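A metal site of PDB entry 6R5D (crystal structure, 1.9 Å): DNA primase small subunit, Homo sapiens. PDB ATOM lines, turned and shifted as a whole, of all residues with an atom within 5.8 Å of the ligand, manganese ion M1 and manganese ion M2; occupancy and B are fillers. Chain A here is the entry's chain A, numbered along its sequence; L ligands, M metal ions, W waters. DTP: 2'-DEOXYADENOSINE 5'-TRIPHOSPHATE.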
ATOM      1  N   TYR A  57       1.025  -9.034  30.513  1.00  0.00           N
ATOM      2  CA  TYR A  57       1.431 -10.432  30.510  1.00  0.00           C
ATOM      3  C   TYR A  57       2.498 -10.678  31.572  1.00  0.00           C
ATOM      4  O   TYR A  57       3.172  -9.751  32.047  1.00  0.00           O
ATOM      5  CB  TYR A  57       1.939 -10.867  29.141  1.00  0.00           C
ATOM      6  CG  TYR A  57       3.209 -10.190  28.675  1.00  0.00           C
ATOM      7  CD1 TYR A  57       3.172  -8.927  28.100  1.00  0.00           C
ATOM      8  CD2 TYR A  57       4.443 -10.807  28.813  1.00  0.00           C
ATOM      9  CE1 TYR A  57       4.323  -8.305  27.667  1.00  0.00           C
ATOM     10  CE2 TYR A  57       5.607 -10.191  28.381  1.00  0.00           C
ATOM     11  CZ  TYR A  57       5.537  -8.943  27.811  1.00  0.00           C
ATOM     12  OH  TYR A  57       6.696  -8.319  27.390  1.00  0.00           O
ATOM     13  N   LYS A  80      -4.730 -15.044  26.555  1.00  0.00           N
ATOM     14  CA  LYS A  80      -4.015 -16.058  25.790  1.00  0.00           C
ATOM     15  C   LYS A  80      -2.907 -16.676  26.638  1.00  0.00           C
ATOM     16  O   LYS A  80      -2.522 -16.150  27.691  1.00  0.00           O
ATOM     17  CB  LYS A  80      -3.431 -15.500  24.480  1.00  0.00           C
ATOM     18  CG  LYS A  80      -2.584 -14.258  24.610  1.00  0.00           C
ATOM     19  CD  LYS A  80      -1.760 -14.019  23.342  1.00  0.00           C
ATOM     20  CE  LYS A  80      -0.358 -14.584  23.491  1.00  0.00           C
ATOM     21  NZ  LYS A  80       0.367 -14.748  22.201  1.00  0.00           N
ATOM     22  N   ASP A  82       0.952 -18.595  26.222  1.00  0.00           N
ATOM     23  CA  ASP A  82       2.139 -18.919  25.431  1.00  0.00           C
ATOM     24  C   ASP A  82       2.958 -19.978  26.151  1.00  0.00           C
ATOM     25  O   ASP A  82       3.043 -19.988  27.388  1.00  0.00           O
ATOM     26  CB  ASP A  82       3.019 -17.689  25.205  1.00  0.00           C
ATOM     27  CG  ASP A  82       2.384 -16.676  24.265  1.00  0.00           C
ATOM     28  OD1 ASP A  82       1.384 -17.013  23.610  1.00  0.00           O
ATOM     29  OD2 ASP A  82       2.902 -15.547  24.189  1.00  0.00           O
ATOM     30  N   ASP A 112       6.185 -20.753  12.677  1.00  0.00           N
ATOM     31  CA  ASP A 112       5.065 -19.812  12.641  1.00  0.00           C
ATOM     32  C   ASP A 112       5.011 -19.229  11.237  1.00  0.00           C
ATOM     33  O   ASP A 112       6.001 -18.666  10.765  1.00  0.00           O
ATOM     34  CB  ASP A 112       5.238 -18.715  13.687  1.00  0.00           C
ATOM     35  CG  ASP A 112       4.215 -17.578  13.527  1.00  0.00           C
ATOM     36  OD1 ASP A 112       3.009 -17.855  13.368  1.00  0.00           O
ATOM     37  OD2 ASP A 112       4.629 -16.405  13.591  1.00  0.00           O
ATOM     38  N   ILE A 113       3.874 -19.396  10.573  1.00  0.00           N
ATOM     39  CA  ILE A 113       3.674 -18.953   9.194  1.00  0.00           C
ATOM     40  C   ILE A 113       2.521 -17.963   9.181  1.00  0.00           C
ATOM     41  O   ILE A 113       1.425 -18.284   9.638  1.00  0.00           O
ATOM     42  CB  ILE A 113       3.392 -20.149   8.254  1.00  0.00           C
ATOM     43  CG1 ILE A 113       4.490 -21.196   8.427  1.00  0.00           C
ATOM     44  CG2 ILE A 113       3.305 -19.668   6.812  1.00  0.00           C
ATOM     45  CD1 ILE A 113       4.349 -22.417   7.530  1.00  0.00           C
ATOM     46  N   ASP A 114       2.777 -16.776   8.629  1.00  0.00           N
ATOM     47  CA  ASP A 114       1.821 -15.675   8.638  1.00  0.00           C
ATOM     48  C   ASP A 114       1.453 -15.308   7.208  1.00  0.00           C
ATOM     49  O   ASP A 114       2.313 -14.926   6.417  1.00  0.00           O
ATOM     50  CB  ASP A 114       2.405 -14.461   9.381  1.00  0.00           C
ATOM     51  CG  ASP A 114       2.663 -14.740  10.844  1.00  0.00           C
ATOM     52  OD1 ASP A 114       1.862 -15.484  11.450  1.00  0.00           O
ATOM     53  OD2 ASP A 114       3.680 -14.225  11.374  1.00  0.00           O
ATOM     54  N   SER A 163      -3.371 -20.906  13.843  1.00  0.00           N
ATOM     55  CA  SER A 163      -3.012 -19.895  14.828  1.00  0.00           C
ATOM     56  C   SER A 163      -4.187 -19.036  15.285  1.00  0.00           C
ATOM     57  O   SER A 163      -4.037 -18.271  16.242  1.00  0.00           O
ATOM     58  CB  SER A 163      -1.892 -19.010  14.292  1.00  0.00           C
ATOM     59  OG  SER A 163      -2.231 -18.440  13.033  1.00  0.00           O
ATOM     60  N   GLY A 164      -5.335 -19.132  14.623  1.00  0.00           N
ATOM     61  CA  GLY A 164      -6.531 -18.445  15.058  1.00  0.00           C
ATOM     62  C   GLY A 164      -6.908 -17.205  14.266  1.00  0.00           C
ATOM     63  O   GLY A 164      -8.017 -16.684  14.450  1.00  0.00           O
ATOM     64  N   ARG A 165      -6.023 -16.712  13.400  1.00  0.00           N
ATOM     65  CA  ARG A 165      -6.340 -15.525  12.627  1.00  0.00           C
ATOM     66  C   ARG A 165      -5.794 -15.586  11.196  1.00  0.00           C
ATOM     67  O   ARG A 165      -6.564 -15.453  10.239  1.00  0.00           O
ATOM     68  CB  ARG A 165      -5.808 -14.266  13.323  1.00  0.00           C
ATOM     69  CG  ARG A 165      -6.163 -12.972  12.588  1.00  0.00           C
ATOM     70  CD  ARG A 165      -5.750 -11.717  13.338  1.00  0.00           C
ATOM     71  NE  ARG A 165      -4.356 -11.747  13.783  1.00  0.00           N
ATOM     72  CZ  ARG A 165      -3.614 -10.674  14.024  1.00  0.00           C
ATOM     73  NH1 ARG A 165      -4.124  -9.455  13.848  1.00  0.00           N
ATOM     74  NH2 ARG A 165      -2.364 -10.807  14.439  1.00  0.00           N
ATOM     75  N   ARG A 166      -4.487 -15.790  11.040  1.00  0.00           N
ATOM     76  CA  ARG A 166      -3.870 -15.556   9.737  1.00  0.00           C
ATOM     77  C   ARG A 166      -2.802 -16.580   9.350  1.00  0.00           C
ATOM     78  O   ARG A 166      -1.958 -16.273   8.509  1.00  0.00           O
ATOM     79  CB  ARG A 166      -3.239 -14.164   9.703  1.00  0.00           C
ATOM     80  CG  ARG A 166      -2.210 -13.993  10.792  1.00  0.00           C
ATOM     81  CD  ARG A 166      -1.238 -12.873  10.522  1.00  0.00           C
ATOM     82  NE  ARG A 166      -0.325 -12.720  11.649  1.00  0.00           N
ATOM     83  CZ  ARG A 166       0.345 -11.606  11.928  1.00  0.00           C
ATOM     84  NH1 ARG A 166       0.193 -10.529  11.174  1.00  0.00           N
ATOM     85  NH2 ARG A 166       1.143 -11.569  12.977  1.00  0.00           N
ATOM     86  N   GLY A 167      -2.802 -17.774   9.941  1.00  0.00           N
ATOM     87  CA  GLY A 167      -1.804 -18.754   9.517  1.00  0.00           C
ATOM     88  C   GLY A 167      -1.820 -20.005  10.354  1.00  0.00           C
ATOM     89  O   GLY A 167      -2.848 -20.386  10.923  1.00  0.00           O
ATOM     90  N   VAL A 168      -0.659 -20.650  10.430  1.00  0.00           N
ATOM     91  CA  VAL A 168      -0.532 -21.939  11.094  1.00  0.00           C
ATOM     92  C   VAL A 168       0.791 -22.012  11.849  1.00  0.00           C
ATOM     93  O   VAL A 168       1.749 -21.285  11.563  1.00  0.00           O
ATOM     94  CB  VAL A 168      -0.627 -23.121  10.099  1.00  0.00           C
ATOM     95  CG1 VAL A 168      -1.952 -23.096   9.358  1.00  0.00           C
ATOM     96  CG2 VAL A 168       0.535 -23.082   9.118  1.00  0.00           C
ATOM     97  N   HIS A 169       0.818 -22.898  12.826  1.00  0.00           N
ATOM     98  CA  HIS A 169       2.011 -23.226  13.590  1.00  0.00           C
ATOM     99  C   HIS A 169       2.318 -24.705  13.380  1.00  0.00           C
ATOM    100  O   HIS A 169       1.432 -25.499  13.060  1.00  0.00           O
ATOM    101  CB  HIS A 169       1.815 -22.981  15.086  1.00  0.00           C
ATOM    102  CG  HIS A 169       1.567 -21.554  15.455  1.00  0.00           C
ATOM    103  ND1 HIS A 169       0.975 -21.197  16.641  1.00  0.00           N
ATOM    104  CD2 HIS A 169       1.817 -20.402  14.793  1.00  0.00           C
ATOM    105  CE1 HIS A 169       0.872 -19.880  16.702  1.00  0.00           C
ATOM    106  NE2 HIS A 169       1.378 -19.372  15.590  1.00  0.00           N
ATOM    107  N   ASP A 309       8.060 -17.204   9.555  1.00  0.00           N
ATOM    108  CA  ASP A 309       8.440 -16.172  10.517  1.00  0.00           C
ATOM    109  C   ASP A 309       9.686 -16.706  11.226  1.00  0.00           C
ATOM    110  O   ASP A 309       9.609 -17.323  12.291  1.00  0.00           O
ATOM    111  CB  ASP A 309       7.299 -15.892  11.483  1.00  0.00           C
ATOM    112  CG  ASP A 309       7.525 -14.641  12.328  1.00  0.00           C
ATOM    113  OD1 ASP A 309       8.691 -14.238  12.500  1.00  0.00           O
ATOM    114  OD2 ASP A 309       6.520 -14.082  12.826  1.00  0.00           O
ATOM    115  N   VAL A 312      10.893 -17.010  15.006  1.00  0.00           N
ATOM    116  CA  VAL A 312      10.169 -17.882  15.916  1.00  0.00           C
ATOM    117  C   VAL A 312      10.910 -19.210  16.087  1.00  0.00           C
ATOM    118  O   VAL A 312      10.861 -19.818  17.159  1.00  0.00           O
ATOM    119  CB  VAL A 312       8.732 -18.105  15.411  1.00  0.00           C
ATOM    120  CG1 VAL A 312       7.958 -19.005  16.353  1.00  0.00           C
ATOM    121  CG2 VAL A 312       8.020 -16.769  15.230  1.00  0.00           C
ATOM    122  N   HIS A 318      12.147 -18.903  22.829  1.00  0.00           N
ATOM    123  CA  HIS A 318      11.058 -18.150  22.214  1.00  0.00           C
ATOM    124  C   HIS A 318       9.693 -18.678  22.642  1.00  0.00           C
ATOM    125  O   HIS A 318       9.399 -19.877  22.525  1.00  0.00           O
ATOM    126  CB  HIS A 318      11.192 -18.209  20.697  1.00  0.00           C
ATOM    127  CG  HIS A 318      10.473 -17.109  19.989  1.00  0.00           C
ATOM    128  ND1 HIS A 318       9.106 -17.089  19.825  1.00  0.00           N
ATOM    129  CD2 HIS A 318      10.931 -15.970  19.403  1.00  0.00           C
ATOM    130  CE1 HIS A 318       8.749 -16.003  19.158  1.00  0.00           C
ATOM    131  NE2 HIS A 318       9.847 -15.310  18.891  1.00  0.00           N
ATOM    132  N   LEU A 319       8.839 -17.766  23.110  1.00  0.00           N
ATOM    133  CA  LEU A 319       7.457 -18.104  23.399  1.00  0.00           C
ATOM    134  C   LEU A 319       6.666 -18.289  22.104  1.00  0.00           C
ATOM    135  O   LEU A 319       6.985 -17.708  21.072  1.00  0.00           O
ATOM    136  CB  LEU A 319       6.812 -16.996  24.246  1.00  0.00           C
ATOM    137  CG  LEU A 319       7.388 -16.787  25.650  1.00  0.00           C
ATOM    138  CD1 LEU A 319       6.946 -15.451  26.216  1.00  0.00           C
ATOM    139  CD2 LEU A 319       6.966 -17.927  26.569  1.00  0.00           C
ATOM    140  N   LEU A 320       5.634 -19.133  22.164  1.00  0.00           N
ATOM    141  CA  LEU A 320       4.702 -19.272  21.063  1.00  0.00           C
ATOM    142  C   LEU A 320       3.323 -19.581  21.612  1.00  0.00           C
ATOM    143  O   LEU A 320       3.192 -20.304  22.602  1.00  0.00           O
ATOM    144  CB  LEU A 320       5.135 -20.370  20.077  1.00  0.00           C
ATOM    145  CG  LEU A 320       4.243 -20.494  18.828  1.00  0.00           C
ATOM    146  CD1 LEU A 320       4.303 -19.220  17.989  1.00  0.00           C
ATOM    147  CD2 LEU A 320       4.638 -21.699  17.990  1.00  0.00           C
ATOM    148  N   LYS A 321       2.292 -19.017  20.970  1.00  0.00           N
ATOM    149  CA  LYS A 321       0.942 -19.200  21.474  1.00  0.00           C
ATOM    150  C   LYS A 321       0.562 -20.674  21.458  1.00  0.00           C
ATOM    151  O   LYS A 321       0.801 -21.398  20.489  1.00  0.00           O
ATOM    152  CB  LYS A 321      -0.067 -18.398  20.642  1.00  0.00           C
ATOM    153  CG  LYS A 321      -1.473 -18.436  21.232  1.00  0.00           C
ATOM    154  CD  LYS A 321      -2.345 -17.298  20.719  1.00  0.00           C
ATOM    155  CE  LYS A 321      -3.248 -17.749  19.579  1.00  0.00           C
ATOM    156  NZ  LYS A 321      -2.484 -18.307  18.441  1.00  0.00           N
ATOM    157  N   HIS A 327      -7.401 -16.919  20.330  1.00  0.00           N
ATOM    158  CA  HIS A 327      -6.804 -15.755  19.684  1.00  0.00           C
ATOM    159  C   HIS A 327      -7.685 -14.560  20.037  1.00  0.00           C
ATOM    160  O   HIS A 327      -8.812 -14.469  19.535  1.00  0.00           O
ATOM    161  CB  HIS A 327      -6.709 -15.936  18.176  1.00  0.00           C
ATOM    162  CG  HIS A 327      -5.790 -14.955  17.520  1.00  0.00           C
ATOM    163  ND1 HIS A 327      -5.924 -13.583  17.686  1.00  0.00           N
ATOM    164  CD2 HIS A 327      -4.724 -15.131  16.705  1.00  0.00           C
ATOM    165  CE1 HIS A 327      -4.982 -12.972  16.999  1.00  0.00           C
ATOM    166  NE2 HIS A 327      -4.232 -13.883  16.394  1.00  0.00           N
HETATM  167  PG  DTP L   1      -1.812 -15.040  14.070  1.00  0.00           P
HETATM  168  O1G DTP L   1      -2.400 -13.694  14.334  1.00  0.00           O
HETATM  169  O2G DTP L   1      -0.566 -14.961  13.233  1.00  0.00           O
HETATM  170  O3G DTP L   1      -2.799 -15.989  13.362  1.00  0.00           O
HETATM  171  PB  DTP L   1      -0.088 -15.943  16.218  1.00  0.00           P
HETATM  172  O1B DTP L   1      -0.342 -16.453  17.576  1.00  0.00           O
HETATM  173  O2B DTP L   1       0.726 -16.894  15.348  1.00  0.00           O
HETATM  174  O3B DTP L   1      -1.481 -15.738  15.468  1.00  0.00           O
HETATM  175  PA  DTP L   1       1.862 -13.808  15.723  1.00  0.00           P
HETATM  176  O1A DTP L   1       1.569 -12.383  15.468  1.00  0.00           O
HETATM  177  O2A DTP L   1       2.198 -14.608  14.447  1.00  0.00           O
HETATM  178  O3A DTP L   1       0.561 -14.499  16.333  1.00  0.00           O
HETATM  179  O5' DTP L   1       2.975 -14.064  16.825  1.00  0.00           O
HETATM  180  C5' DTP L   1       3.516 -15.391  16.933  1.00  0.00           C
HETATM  181  C4' DTP L   1       4.370 -15.555  18.148  1.00  0.00           C
HETATM  182  O4' DTP L   1       5.302 -14.456  18.298  1.00  0.00           O
HETATM  183  C3' DTP L   1       3.676 -15.598  19.503  1.00  0.00           C
HETATM  184  O3' DTP L   1       2.937 -16.786  19.733  1.00  0.00           O
HETATM  185  C2' DTP L   1       4.895 -15.484  20.402  1.00  0.00           C
HETATM  186  C1' DTP L   1       5.648 -14.373  19.685  1.00  0.00           C
HETATM  187  N9  DTP L   1       5.252 -13.066  20.210  1.00  0.00           N
HETATM  188  C8  DTP L   1       4.416 -12.101  19.715  1.00  0.00           C
HETATM  189  N7  DTP L   1       4.263 -11.070  20.523  1.00  0.00           N
HETATM  190  C5  DTP L   1       5.020 -11.415  21.630  1.00  0.00           C
HETATM  191  C6  DTP L   1       5.290 -10.736  22.845  1.00  0.00           C
HETATM  192  N6  DTP L   1       4.780  -9.539  23.158  1.00  0.00           N
HETATM  193  N1  DTP L   1       6.091 -11.353  23.743  1.00  0.00           N
HETATM  194  C2  DTP L   1       6.595 -12.543  23.441  1.00  0.00           C
HETATM  195  N3  DTP L   1       6.423 -13.275  22.329  1.00  0.00           N
HETATM  196  C4  DTP L   1       5.618 -12.642  21.465  1.00  0.00           C
HETATM  197 MN    MN M   1       4.442 -14.282  13.417  1.00  0.00          MN
HETATM  198 MN    MN M   2       1.446 -16.267  13.390  1.00  0.00          MN
HETATM  199  O   HOH W   1       5.727 -13.802  15.589  1.00  0.00           O
HETATM  200  O   HOH W   2       9.371 -14.742  22.802  1.00  0.00           O
HETATM  201  O   HOH W   3       0.499 -17.738  12.440  1.00  0.00           O
HETATM  202  O   HOH W   4       0.386 -14.885  19.530  1.00  0.00           O
HETATM  203  O   HOH W   5       4.454 -11.879  14.132  1.00  0.00           O
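Water W3 lies within hydrogen-bond range of OG of Ser 163 (2.9 Å) and O of Ile 113 (3.0 Å). Water W4 bridges an oxygen (O1B) of the ligand and the side-chain amino group (NZ) of Lys 80. Water W2 bridges the backbone NH of Leu 319 (3.1 Å) and a nitrogen (N3) of the ligand (3.3 Å).
Manganese ion M2 is bound by water W3 (2.0 Å). O2A of the ligand is bound to manganese ion M2. OD1 of Asp 114 is bound to manganese ion M2 (2.1 Å). O2B of the ligand is bound to manganese ion M2, at 2.2 Å. OD1 of Asp 112 binds manganese ion M2 (2.2 Å). O2G of the ligand is bound to manganese ion M2, at 2.4 Å.
An oxygen (O3') of the ligand sits at hydrogen-bond distance from the backbone NH of Lys 321. O3G of the ligand lies within hydrogen-bond range of OG of Ser 163 (2.5 Å). An oxygen (O1B) of the ligand lies within salt-bridge range of the side-chain amino group (NZ) of Lys 321 (3.0 Å). The backbone NH of Arg 165 sits at hydrogen-bond distance from an oxygen (O3G) of the ligand, at 3.3 Å. A ring nitrogen (NE2) of His 169 sits close to an oxygen (O2B) of the ligand (2.6 Å). NE2 of His 327 is in hydrogen-bond range of O1G of the ligand, at 2.8 Å. NH2 of Arg 166 is in salt-bridge range of O1A of the ligand, at 2.7 Å. O3G of the ligand lies within hydrogen-bond range of N of Arg 166 (2.9 Å). An oxygen (O1G) of the ligand lies within salt-bridge range of the guanidinium group (NE) of Arg 165, at 2.8 Å.
Three residues have an atom within 4 Å of manganese ion M1: Asp 112, Asp 114 and Asp 309. The nearest printed residue that does not touch manganese ion M1 is Arg 166 (4.3 Å).
Merely in contact with manganese ion M2: His 169.
Manganese ion M1 is bound by OD2 of Asp 112 (2.1 Å), OD2 of Asp 309 (2.2 Å), OD2 of Asp 114 (2.2 Å), O2A of the ligand (2.5 Å), water W5 (2.5 Å) and water W1 (2.6 Å). Manganese ion M1 has six donor atoms within binding distance.
Merely in contact with the ligand: Gly 167 (3.9 Å), His 318 (3.5 Å), Leu 319 (3.1 Å) and Leu 320 (3.3 Å). Of the 20 residues printed, 12 come within 4 Å of the ligand. The nearest printed residue that does not touch the ligand is Lys 80 (4.1 Å).
N of Lys 321 sits close to OD1 of Asp 82. NE of Arg 166 lies close to OD1 of Asp 114 (3.5 Å). The side-chain hydroxyl of Ser 163 sits at hydrogen-bond distance from the backbone carbonyl oxygen of Gly 167 (2.9 Å). NE of Arg 165 sits at hydrogen-bond distance from NE2 of His 327. O of Ser 163 is in hydrogen-bond range of NZ of Lys 321. OD1 of Asp 112 lies close to NE2 of His 169 (3.1 Å).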
